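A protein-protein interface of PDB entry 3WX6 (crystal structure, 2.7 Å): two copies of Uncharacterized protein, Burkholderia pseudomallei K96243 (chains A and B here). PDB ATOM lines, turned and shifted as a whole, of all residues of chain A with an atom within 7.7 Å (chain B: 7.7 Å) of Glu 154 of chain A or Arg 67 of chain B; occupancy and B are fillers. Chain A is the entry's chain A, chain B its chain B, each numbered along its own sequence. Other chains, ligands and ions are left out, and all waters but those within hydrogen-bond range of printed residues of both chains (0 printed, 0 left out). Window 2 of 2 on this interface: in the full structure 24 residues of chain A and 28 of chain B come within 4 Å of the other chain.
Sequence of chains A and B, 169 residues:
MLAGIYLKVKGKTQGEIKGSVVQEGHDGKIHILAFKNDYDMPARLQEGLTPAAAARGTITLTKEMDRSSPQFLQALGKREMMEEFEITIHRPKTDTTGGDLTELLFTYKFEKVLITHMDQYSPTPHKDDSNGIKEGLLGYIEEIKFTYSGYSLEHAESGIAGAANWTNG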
ATOM      1  N   ILE A  87      12.708  -4.052  22.823  1.00  0.00           N
ATOM      2  CA  ILE A  87      13.380  -5.234  22.323  1.00  0.00           C
ATOM      3  C   ILE A  87      13.755  -6.130  23.500  1.00  0.00           C
ATOM      4  O   ILE A  87      14.538  -5.725  24.362  1.00  0.00           O
ATOM      5  CB  ILE A  87      14.650  -4.860  21.517  1.00  0.00           C
ATOM      6  CG1 ILE A  87      14.304  -4.401  20.093  1.00  0.00           C
ATOM      7  CG2 ILE A  87      15.597  -6.035  21.437  1.00  0.00           C
ATOM      8  CD1 ILE A  87      13.787  -5.497  19.189  1.00  0.00           C
ATOM      9  N   THR A  88      13.156  -7.315  23.581  1.00  0.00           N
ATOM     10  CA  THR A  88      13.494  -8.239  24.662  1.00  0.00           C
ATOM     11  C   THR A  88      14.441  -9.255  24.051  1.00  0.00           C
ATOM     12  O   THR A  88      14.261  -9.694  22.915  1.00  0.00           O
ATOM     13  CB  THR A  88      12.251  -8.908  25.296  1.00  0.00           C
ATOM     14  OG1 THR A  88      12.650  -9.721  26.407  1.00  0.00           O
ATOM     15  CG2 THR A  88      11.532  -9.757  24.309  1.00  0.00           C
ATOM     16  N   ILE A  89      15.475  -9.597  24.804  1.00  0.00           N
ATOM     17  CA  ILE A  89      16.669 -10.118  24.175  1.00  0.00           C
ATOM     18  C   ILE A  89      17.451 -11.111  25.025  1.00  0.00           C
ATOM     19  O   ILE A  89      16.873 -11.986  25.656  1.00  0.00           O
ATOM     20  CB  ILE A  89      17.570  -8.919  23.769  1.00  0.00           C
ATOM     21  CG1 ILE A  89      18.152  -9.119  22.374  1.00  0.00           C
ATOM     22  CG2 ILE A  89      18.582  -8.582  24.830  1.00  0.00           C
ATOM     23  CD1 ILE A  89      17.083  -9.268  21.337  1.00  0.00           C
ATOM     24  N   LEU A 105       7.774  -5.742  29.511  1.00  0.00           N
ATOM     25  CA  LEU A 105       8.600  -6.901  29.830  1.00  0.00           C
ATOM     26  C   LEU A 105       9.693  -7.118  28.787  1.00  0.00           C
ATOM     27  O   LEU A 105       9.444  -7.740  27.751  1.00  0.00           O
ATOM     28  CB  LEU A 105       7.734  -8.157  29.940  1.00  0.00           C
ATOM     29  N   PHE A 106      10.899  -6.618  29.068  1.00  0.00           N
ATOM     30  CA  PHE A 106      12.017  -6.729  28.124  1.00  0.00           C
ATOM     31  C   PHE A 106      13.375  -6.272  28.649  1.00  0.00           C
ATOM     32  O   PHE A 106      13.725  -6.492  29.802  1.00  0.00           O
ATOM     33  CB  PHE A 106      11.715  -5.930  26.859  1.00  0.00           C
ATOM     34  N   THR A 107      14.123  -5.626  27.760  1.00  0.00           N
ATOM     35  CA  THR A 107      15.497  -5.194  27.998  1.00  0.00           C
ATOM     36  C   THR A 107      15.881  -3.895  27.327  1.00  0.00           C
ATOM     37  O   THR A 107      16.180  -2.907  27.990  1.00  0.00           O
ATOM     38  CB  THR A 107      16.503  -6.223  27.510  1.00  0.00           C
ATOM     39  OG1 THR A 107      16.117  -7.533  27.944  1.00  0.00           O
ATOM     40  CG2 THR A 107      17.859  -5.859  28.042  1.00  0.00           C
ATOM     41  N   TYR A 108      15.879  -3.908  26.001  1.00  0.00           N
ATOM     42  CA  TYR A 108      16.101  -2.691  25.262  1.00  0.00           C
ATOM     43  C   TYR A 108      14.762  -1.996  25.130  1.00  0.00           C
ATOM     44  O   TYR A 108      13.771  -2.603  24.731  1.00  0.00           O
ATOM     45  CB  TYR A 108      16.678  -2.991  23.881  1.00  0.00           C
ATOM     46  CG  TYR A 108      18.148  -3.309  23.829  1.00  0.00           C
ATOM     47  CD1 TYR A 108      19.089  -2.301  23.770  1.00  0.00           C
ATOM     48  CD2 TYR A 108      18.591  -4.617  23.826  1.00  0.00           C
ATOM     49  CE1 TYR A 108      20.434  -2.581  23.705  1.00  0.00           C
ATOM     50  CE2 TYR A 108      19.932  -4.911  23.766  1.00  0.00           C
ATOM     51  CZ  TYR A 108      20.852  -3.888  23.701  1.00  0.00           C
ATOM     52  OH  TYR A 108      22.196  -4.169  23.643  1.00  0.00           O
ATOM     53  N   LYS A 109      14.748  -0.714  25.460  1.00  0.00           N
ATOM     54  CA  LYS A 109      13.595   0.127  25.232  1.00  0.00           C
ATOM     55  C   LYS A 109      14.144   1.430  24.714  1.00  0.00           C
ATOM     56  O   LYS A 109      15.146   1.926  25.219  1.00  0.00           O
ATOM     57  CB  LYS A 109      12.776   0.301  26.515  1.00  0.00           C
ATOM     58  CG  LYS A 109      12.218  -1.008  27.030  1.00  0.00           C
ATOM     59  CD  LYS A 109      11.947  -0.996  28.519  1.00  0.00           C
ATOM     60  CE  LYS A 109      11.090   0.185  28.907  1.00  0.00           C
ATOM     61  NZ  LYS A 109      10.268  -0.120  30.107  1.00  0.00           N
ATOM     62  N   SER A 152      17.229   2.442  27.199  1.00  0.00           N
ATOM     63  CA  SER A 152      17.422   1.712  28.449  1.00  0.00           C
ATOM     64  C   SER A 152      17.782   0.255  28.166  1.00  0.00           C
ATOM     65  O   SER A 152      17.137  -0.394  27.354  1.00  0.00           O
ATOM     66  CB  SER A 152      16.169   1.799  29.323  1.00  0.00           C
ATOM     67  OG  SER A 152      16.395   1.211  30.591  1.00  0.00           O
ATOM     68  N   LEU A 153      18.841  -0.230  28.807  1.00  0.00           N
ATOM     69  CA  LEU A 153      19.235  -1.640  28.742  1.00  0.00           C
ATOM     70  C   LEU A 153      19.172  -2.241  30.151  1.00  0.00           C
ATOM     71  O   LEU A 153      19.582  -1.594  31.113  1.00  0.00           O
ATOM     72  CB  LEU A 153      20.643  -1.763  28.124  1.00  0.00           C
ATOM     73  CG  LEU A 153      21.350  -3.111  27.934  1.00  0.00           C
ATOM     74  CD1 LEU A 153      20.572  -4.005  27.012  1.00  0.00           C
ATOM     75  CD2 LEU A 153      22.771  -2.923  27.422  1.00  0.00           C
ATOM     76  N   GLU A 154      18.669  -3.467  30.286  1.00  0.00           N
ATOM     77  CA  GLU A 154      18.514  -4.056  31.617  1.00  0.00           C
ATOM     78  C   GLU A 154      18.998  -5.497  31.689  1.00  0.00           C
ATOM     79  O   GLU A 154      18.392  -6.389  31.110  1.00  0.00           O
ATOM     80  CB  GLU A 154      17.048  -3.984  32.059  1.00  0.00           C
ATOM     81  N   ILE A 160      21.703  -4.984  36.876  1.00  0.00           N
ATOM     82  CA  ILE A 160      21.939  -3.585  36.577  1.00  0.00           C
ATOM     83  C   ILE A 160      21.171  -3.097  35.343  1.00  0.00           C
ATOM     84  O   ILE A 160      21.036  -3.814  34.351  1.00  0.00           O
ATOM     85  CB  ILE A 160      23.439  -3.278  36.370  1.00  0.00           C
ATOM     86  CG1 ILE A 160      24.288  -3.665  37.594  1.00  0.00           C
ATOM     87  CG2 ILE A 160      23.624  -1.803  36.181  1.00  0.00           C
ATOM     88  CD1 ILE A 160      24.511  -5.143  37.851  1.00  0.00           C
ATOM     89  N   ALA A 161      20.618  -1.894  35.434  1.00  0.00           N
ATOM     90  CA  ALA A 161      19.918  -1.295  34.311  1.00  0.00           C
ATOM     91  C   ALA A 161      20.578   0.043  34.014  1.00  0.00           C
ATOM     92  O   ALA A 161      20.867   0.818  34.924  1.00  0.00           O
ATOM     93  CB  ALA A 161      18.449  -1.115  34.612  1.00  0.00           C
ATOM     94  N   GLY A 162      20.843   0.299  32.739  1.00  0.00           N
ATOM     95  CA  GLY A 162      21.368   1.581  32.308  1.00  0.00           C
ATOM     96  C   GLY A 162      20.354   2.365  31.500  1.00  0.00           C
ATOM     97  O   GLY A 162      19.505   1.772  30.835  1.00  0.00           O
ATOM     98  N   ALA A 163      20.429   3.692  31.569  1.00  0.00           N
ATOM     99  CA  ALA A 163      19.501   4.553  30.845  1.00  0.00           C
ATOM    100  C   ALA A 163      20.074   5.954  30.656  1.00  0.00           C
ATOM    101  O   ALA A 163      20.697   6.500  31.567  1.00  0.00           O
ATOM    102  CB  ALA A 163      18.172   4.620  31.575  1.00  0.00           C
ATOM    103  N   GLY B  15       9.700 -18.875  29.310  1.00  0.00           N
ATOM    104  CA  GLY B  15       9.687 -17.459  29.630  1.00  0.00           C
ATOM    105  C   GLY B  15      10.897 -16.618  29.289  1.00  0.00           C
ATOM    106  O   GLY B  15      11.550 -16.095  30.190  1.00  0.00           O
ATOM    107  N   GLU B  16      11.204 -16.484  28.002  1.00  0.00           N
ATOM    108  CA  GLU B  16      12.331 -15.652  27.586  1.00  0.00           C
ATOM    109  C   GLU B  16      11.985 -14.201  27.256  1.00  0.00           C
ATOM    110  O   GLU B  16      12.734 -13.539  26.544  1.00  0.00           O
ATOM    111  CB  GLU B  16      13.068 -16.278  26.397  1.00  0.00           C
ATOM    112  CG  GLU B  16      13.208 -17.791  26.403  1.00  0.00           C
ATOM    113  CD  GLU B  16      12.009 -18.520  25.870  1.00  0.00           C
ATOM    114  OE1 GLU B  16      11.436 -18.066  24.862  1.00  0.00           O
ATOM    115  OE2 GLU B  16      11.659 -19.568  26.445  1.00  0.00           O
ATOM    116  N   ILE B  17      10.866 -13.707  27.776  1.00  0.00           N
ATOM    117  CA  ILE B  17      10.388 -12.376  27.424  1.00  0.00           C
ATOM    118  C   ILE B  17       9.907 -12.282  25.983  1.00  0.00           C
ATOM    119  O   ILE B  17      10.665 -12.555  25.055  1.00  0.00           O
ATOM    120  N   LYS B  63      20.559 -11.311  17.392  1.00  0.00           N
ATOM    121  CA  LYS B  63      19.935 -10.482  18.430  1.00  0.00           C
ATOM    122  C   LYS B  63      20.985 -10.073  19.464  1.00  0.00           C
ATOM    123  O   LYS B  63      22.047 -10.672  19.508  1.00  0.00           O
ATOM    124  CB  LYS B  63      18.789 -11.233  19.119  1.00  0.00           C
ATOM    125  CG  LYS B  63      19.246 -12.221  20.190  1.00  0.00           C
ATOM    126  CD  LYS B  63      18.073 -12.905  20.884  1.00  0.00           C
ATOM    127  CE  LYS B  63      18.490 -13.534  22.210  1.00  0.00           C
ATOM    128  NZ  LYS B  63      19.894 -14.029  22.196  1.00  0.00           N
ATOM    129  N   MET B  65      21.736  -9.500  23.789  1.00  0.00           N
ATOM    130  CA  MET B  65      21.740 -10.521  24.848  1.00  0.00           C
ATOM    131  C   MET B  65      21.060 -10.117  26.177  1.00  0.00           C
ATOM    132  O   MET B  65      21.254  -9.011  26.684  1.00  0.00           O
ATOM    133  CB  MET B  65      23.188 -10.977  25.113  1.00  0.00           C
ATOM    134  CG  MET B  65      23.760 -11.865  24.003  1.00  0.00           C
ATOM    135  SD  MET B  65      25.709 -12.077  23.876  1.00  0.00           S
ATOM    136  CE  MET B  65      26.104 -12.820  25.636  1.00  0.00           C
ATOM    137  N   ASP B  66      20.231 -11.027  26.693  1.00  0.00           N
ATOM    138  CA  ASP B  66      19.569 -10.920  28.001  1.00  0.00           C
ATOM    139  C   ASP B  66      19.079 -12.223  28.569  1.00  0.00           C
ATOM    140  O   ASP B  66      19.745 -13.240  28.501  1.00  0.00           O
ATOM    141  CB  ASP B  66      18.359  -9.997  27.985  1.00  0.00           C
ATOM    142  CG  ASP B  66      18.543  -8.802  28.854  1.00  0.00           C
ATOM    143  OD1 ASP B  66      19.678  -8.303  28.979  1.00  0.00           O
ATOM    144  OD2 ASP B  66      17.545  -8.410  29.488  1.00  0.00           O
ATOM    145  N   ARG B  67      17.869 -12.141  29.113  1.00  0.00           N
ATOM    146  CA  ARG B  67      17.211 -13.203  29.857  1.00  0.00           C
ATOM    147  C   ARG B  67      16.991 -14.471  29.056  1.00  0.00           C
ATOM    148  O   ARG B  67      16.758 -15.533  29.623  1.00  0.00           O
ATOM    149  CB  ARG B  67      15.864 -12.682  30.343  1.00  0.00           C
ATOM    150  CG  ARG B  67      15.918 -11.180  30.546  1.00  0.00           C
ATOM    151  CD  ARG B  67      14.566 -10.498  30.621  1.00  0.00           C
ATOM    152  NE  ARG B  67      14.736  -9.043  30.677  1.00  0.00           N
ATOM    153  CZ  ARG B  67      15.388  -8.366  31.627  1.00  0.00           C
ATOM    154  NH1 ARG B  67      15.916  -8.981  32.677  1.00  0.00           N
ATOM    155  NH2 ARG B  67      15.483  -7.044  31.540  1.00  0.00           N
ATOM    156  N   SER B  68      17.101 -14.367  27.738  1.00  0.00           N
ATOM    157  CA  SER B  68      16.849 -15.505  26.877  1.00  0.00           C
ATOM    158  C   SER B  68      18.163 -16.151  26.488  1.00  0.00           C
ATOM    159  O   SER B  68      18.233 -17.344  26.195  1.00  0.00           O
ATOM    160  CB  SER B  68      16.072 -15.057  25.645  1.00  0.00           C
ATOM    161  OG  SER B  68      16.796 -14.104  24.900  1.00  0.00           O
ATOM    162  N   SER B  69      19.208 -15.337  26.497  1.00  0.00           N
ATOM    163  CA  SER B  69      20.549 -15.803  26.204  1.00  0.00           C
ATOM    164  C   SER B  69      20.946 -17.033  27.025  1.00  0.00           C
ATOM    165  O   SER B  69      21.373 -18.027  26.447  1.00  0.00           O
ATOM    166  CB  SER B  69      21.560 -14.682  26.410  1.00  0.00           C
ATOM    167  OG  SER B  69      21.411 -13.699  25.410  1.00  0.00           O
ATOM    168  N   PRO B  70      20.802 -16.988  28.371  1.00  0.00           N
ATOM    169  CA  PRO B  70      21.188 -18.196  29.099  1.00  0.00           C
ATOM    170  C   PRO B  70      20.206 -19.310  28.841  1.00  0.00           C
ATOM    171  O   PRO B  70      20.560 -20.489  28.896  1.00  0.00           O
ATOM    172  CB  PRO B  70      21.131 -17.762  30.563  1.00  0.00           C
ATOM    173  CG  PRO B  70      21.087 -16.284  30.544  1.00  0.00           C
ATOM    174  CD  PRO B  70      20.356 -15.944  29.305  1.00  0.00           C
ATOM    175  N   GLN B  71      18.975 -18.915  28.539  1.00  0.00           N
ATOM    176  CA  GLN B  71      17.915 -19.860  28.245  1.00  0.00           C
ATOM    177  C   GLN B  71      18.145 -20.501  26.885  1.00  0.00           C
ATOM    178  O   GLN B  71      17.924 -21.700  26.724  1.00  0.00           O
ATOM    179  CB  GLN B  71      16.551 -19.179  28.321  1.00  0.00           C
ATOM    180  CG  GLN B  71      16.180 -18.725  29.730  1.00  0.00           C
ATOM    181  CD  GLN B  71      14.833 -18.050  29.821  1.00  0.00           C
ATOM    182  OE1 GLN B  71      14.599 -17.025  29.192  1.00  0.00           O
ATOM    183  NE2 GLN B  71      13.936 -18.627  30.609  1.00  0.00           N
ATOM    184  N   PHE B  72      18.591 -19.716  25.908  1.00  0.00           N
ATOM    185  CA  PHE B  72      18.971 -20.308  24.633  1.00  0.00           C
ATOM    186  C   PHE B  72      20.228 -21.151  24.745  1.00  0.00           C
ATOM    187  O   PHE B  72      20.311 -22.228  24.159  1.00  0.00           O
ATOM    188  CB  PHE B  72      19.211 -19.250  23.558  1.00  0.00           C
ATOM    189  CG  PHE B  72      17.984 -18.533  23.105  1.00  0.00           C
ATOM    190  CD1 PHE B  72      17.026 -19.207  22.387  1.00  0.00           C
ATOM    191  CD2 PHE B  72      17.832 -17.173  23.292  1.00  0.00           C
ATOM    192  CE1 PHE B  72      15.916 -18.560  21.929  1.00  0.00           C
ATOM    193  CE2 PHE B  72      16.710 -16.520  22.823  1.00  0.00           C
ATOM    194  CZ  PHE B  72      15.750 -17.214  22.146  1.00  0.00           C
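Of chain B, only Asp 66 (2.7 Å) and Arg 67 (3.0 Å) come within 4 Å of Glu 154 of chain A.
Of the printed residues of chain A, Arg 67 of chain B touches Ile 89, Phe 106, Thr 107 and Glu 154.
Asp 66 of chain B touches just these residues of chain A: Ile 89 (3.2 Å), Thr 107 (2.3 Å) and Glu 154 (2.7 Å).
Printed residues of chain A within 4 Å of Glu 16 of chain B: Thr 88 (3.8 Å).
Printed residues of chain A within 4 Å of Ile 17 of chain B: Thr 88.
Gly 15 of chain B touches none of the printed residues of chain A.
Leu 153 of chain A touches none of the printed residues of chain B.
The nearest residue of chain A that does not touch Arg 67 of chain B is Thr 88 of chain A (4.7 Å).
Hydrophobic or aromatic side chains of chain A within 4 Å of the printed part of chain B: Ile 89.
Along chain A the printed residues that touch a printed residue of chain B span positions 88 to 154.
Printed residues of chain B that touch a printed residue of chain A: Glu 16, Ile 17, Lys 63, Met 65, Asp 66, Arg 67 and Ser 68.
Among the printed residues, 12 pairs touch across the chains.
Among the printed residues, no Asp or Glu carboxylate lies within 4 Å of a Lys or Arg side-chain nitrogen of the other chain.
Thr 88 of chain A touches Glu 16 of chain B (OG1 to O, 3.8 Å).
Thr 88 of chain A touches Ile 17 of chain B (CG2 to O, 3.0 Å).
Ile 89 of chain A touches Lys 63 of chain B.
CG2 of Ile 89 of chain A touches C of Met 65 of chain B (3.2 Å).
C of Ile 89 of chain A touches N of Asp 66 of chain B, 3.2 Å away.
Arg 67 of chain B touches Ile 89 of chain A (N to O, 3.6 Å).
The backbone carbonyl oxygen (O) of Ile 87 of chain A lies within hydrogen-bond range of the backbone NH (N) of Thr 107 of chain A.
The backbone NH (N) of Glu 154 of chain A lies close to the backbone carbonyl oxygen (O) of Thr 107 of chain A (3.4 Å).
The side-chain carboxylate (OD2) of Asp 66 of chain B lies within salt-bridge range of the guanidinium group (NE) of Arg 67 of chain B, 3.1 Å away.
The backbone NH of Asp 66 of chain B sits at hydrogen-bond distance from the side-chain hydroxyl of Ser 69 of chain B, at 3.2 Å.
OE1 of Gln 71 of chain B lies close to O of Arg 67 of chain B (2.7 Å).
O of Ile 89 of chain A lies within hydrogen-bond range of N of Ser 68 of chain B, at 3.2 Å.
NH2 of Arg 67 of chain B is in hydrogen-bond range of O of Phe 106 of chain A (2.5 Å).
The side-chain hydroxyl of Thr 107 of chain A sits at hydrogen-bond distance from the guanidinium group of Arg 67 of chain B (3.4 Å).
The side-chain carboxylate (OD2) of Asp 66 of chain B sits close to the backbone carbonyl oxygen (O) of Glu 154 of chain A, at 2.7 Å.
The backbone carbonyl oxygen of Glu 154 of chain A sits at hydrogen-bond distance from the guanidinium group of Arg 67 of chain B (3.0 Å).
OD2 of Asp 66 of chain B sits close to OG1 of Thr 107 of chain A, 2.3 Å away.
No position is printed for both chains.
Of the 12 pairs that touch across the chains among the printed residues, none has its exchanged pair printed and touching as well.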
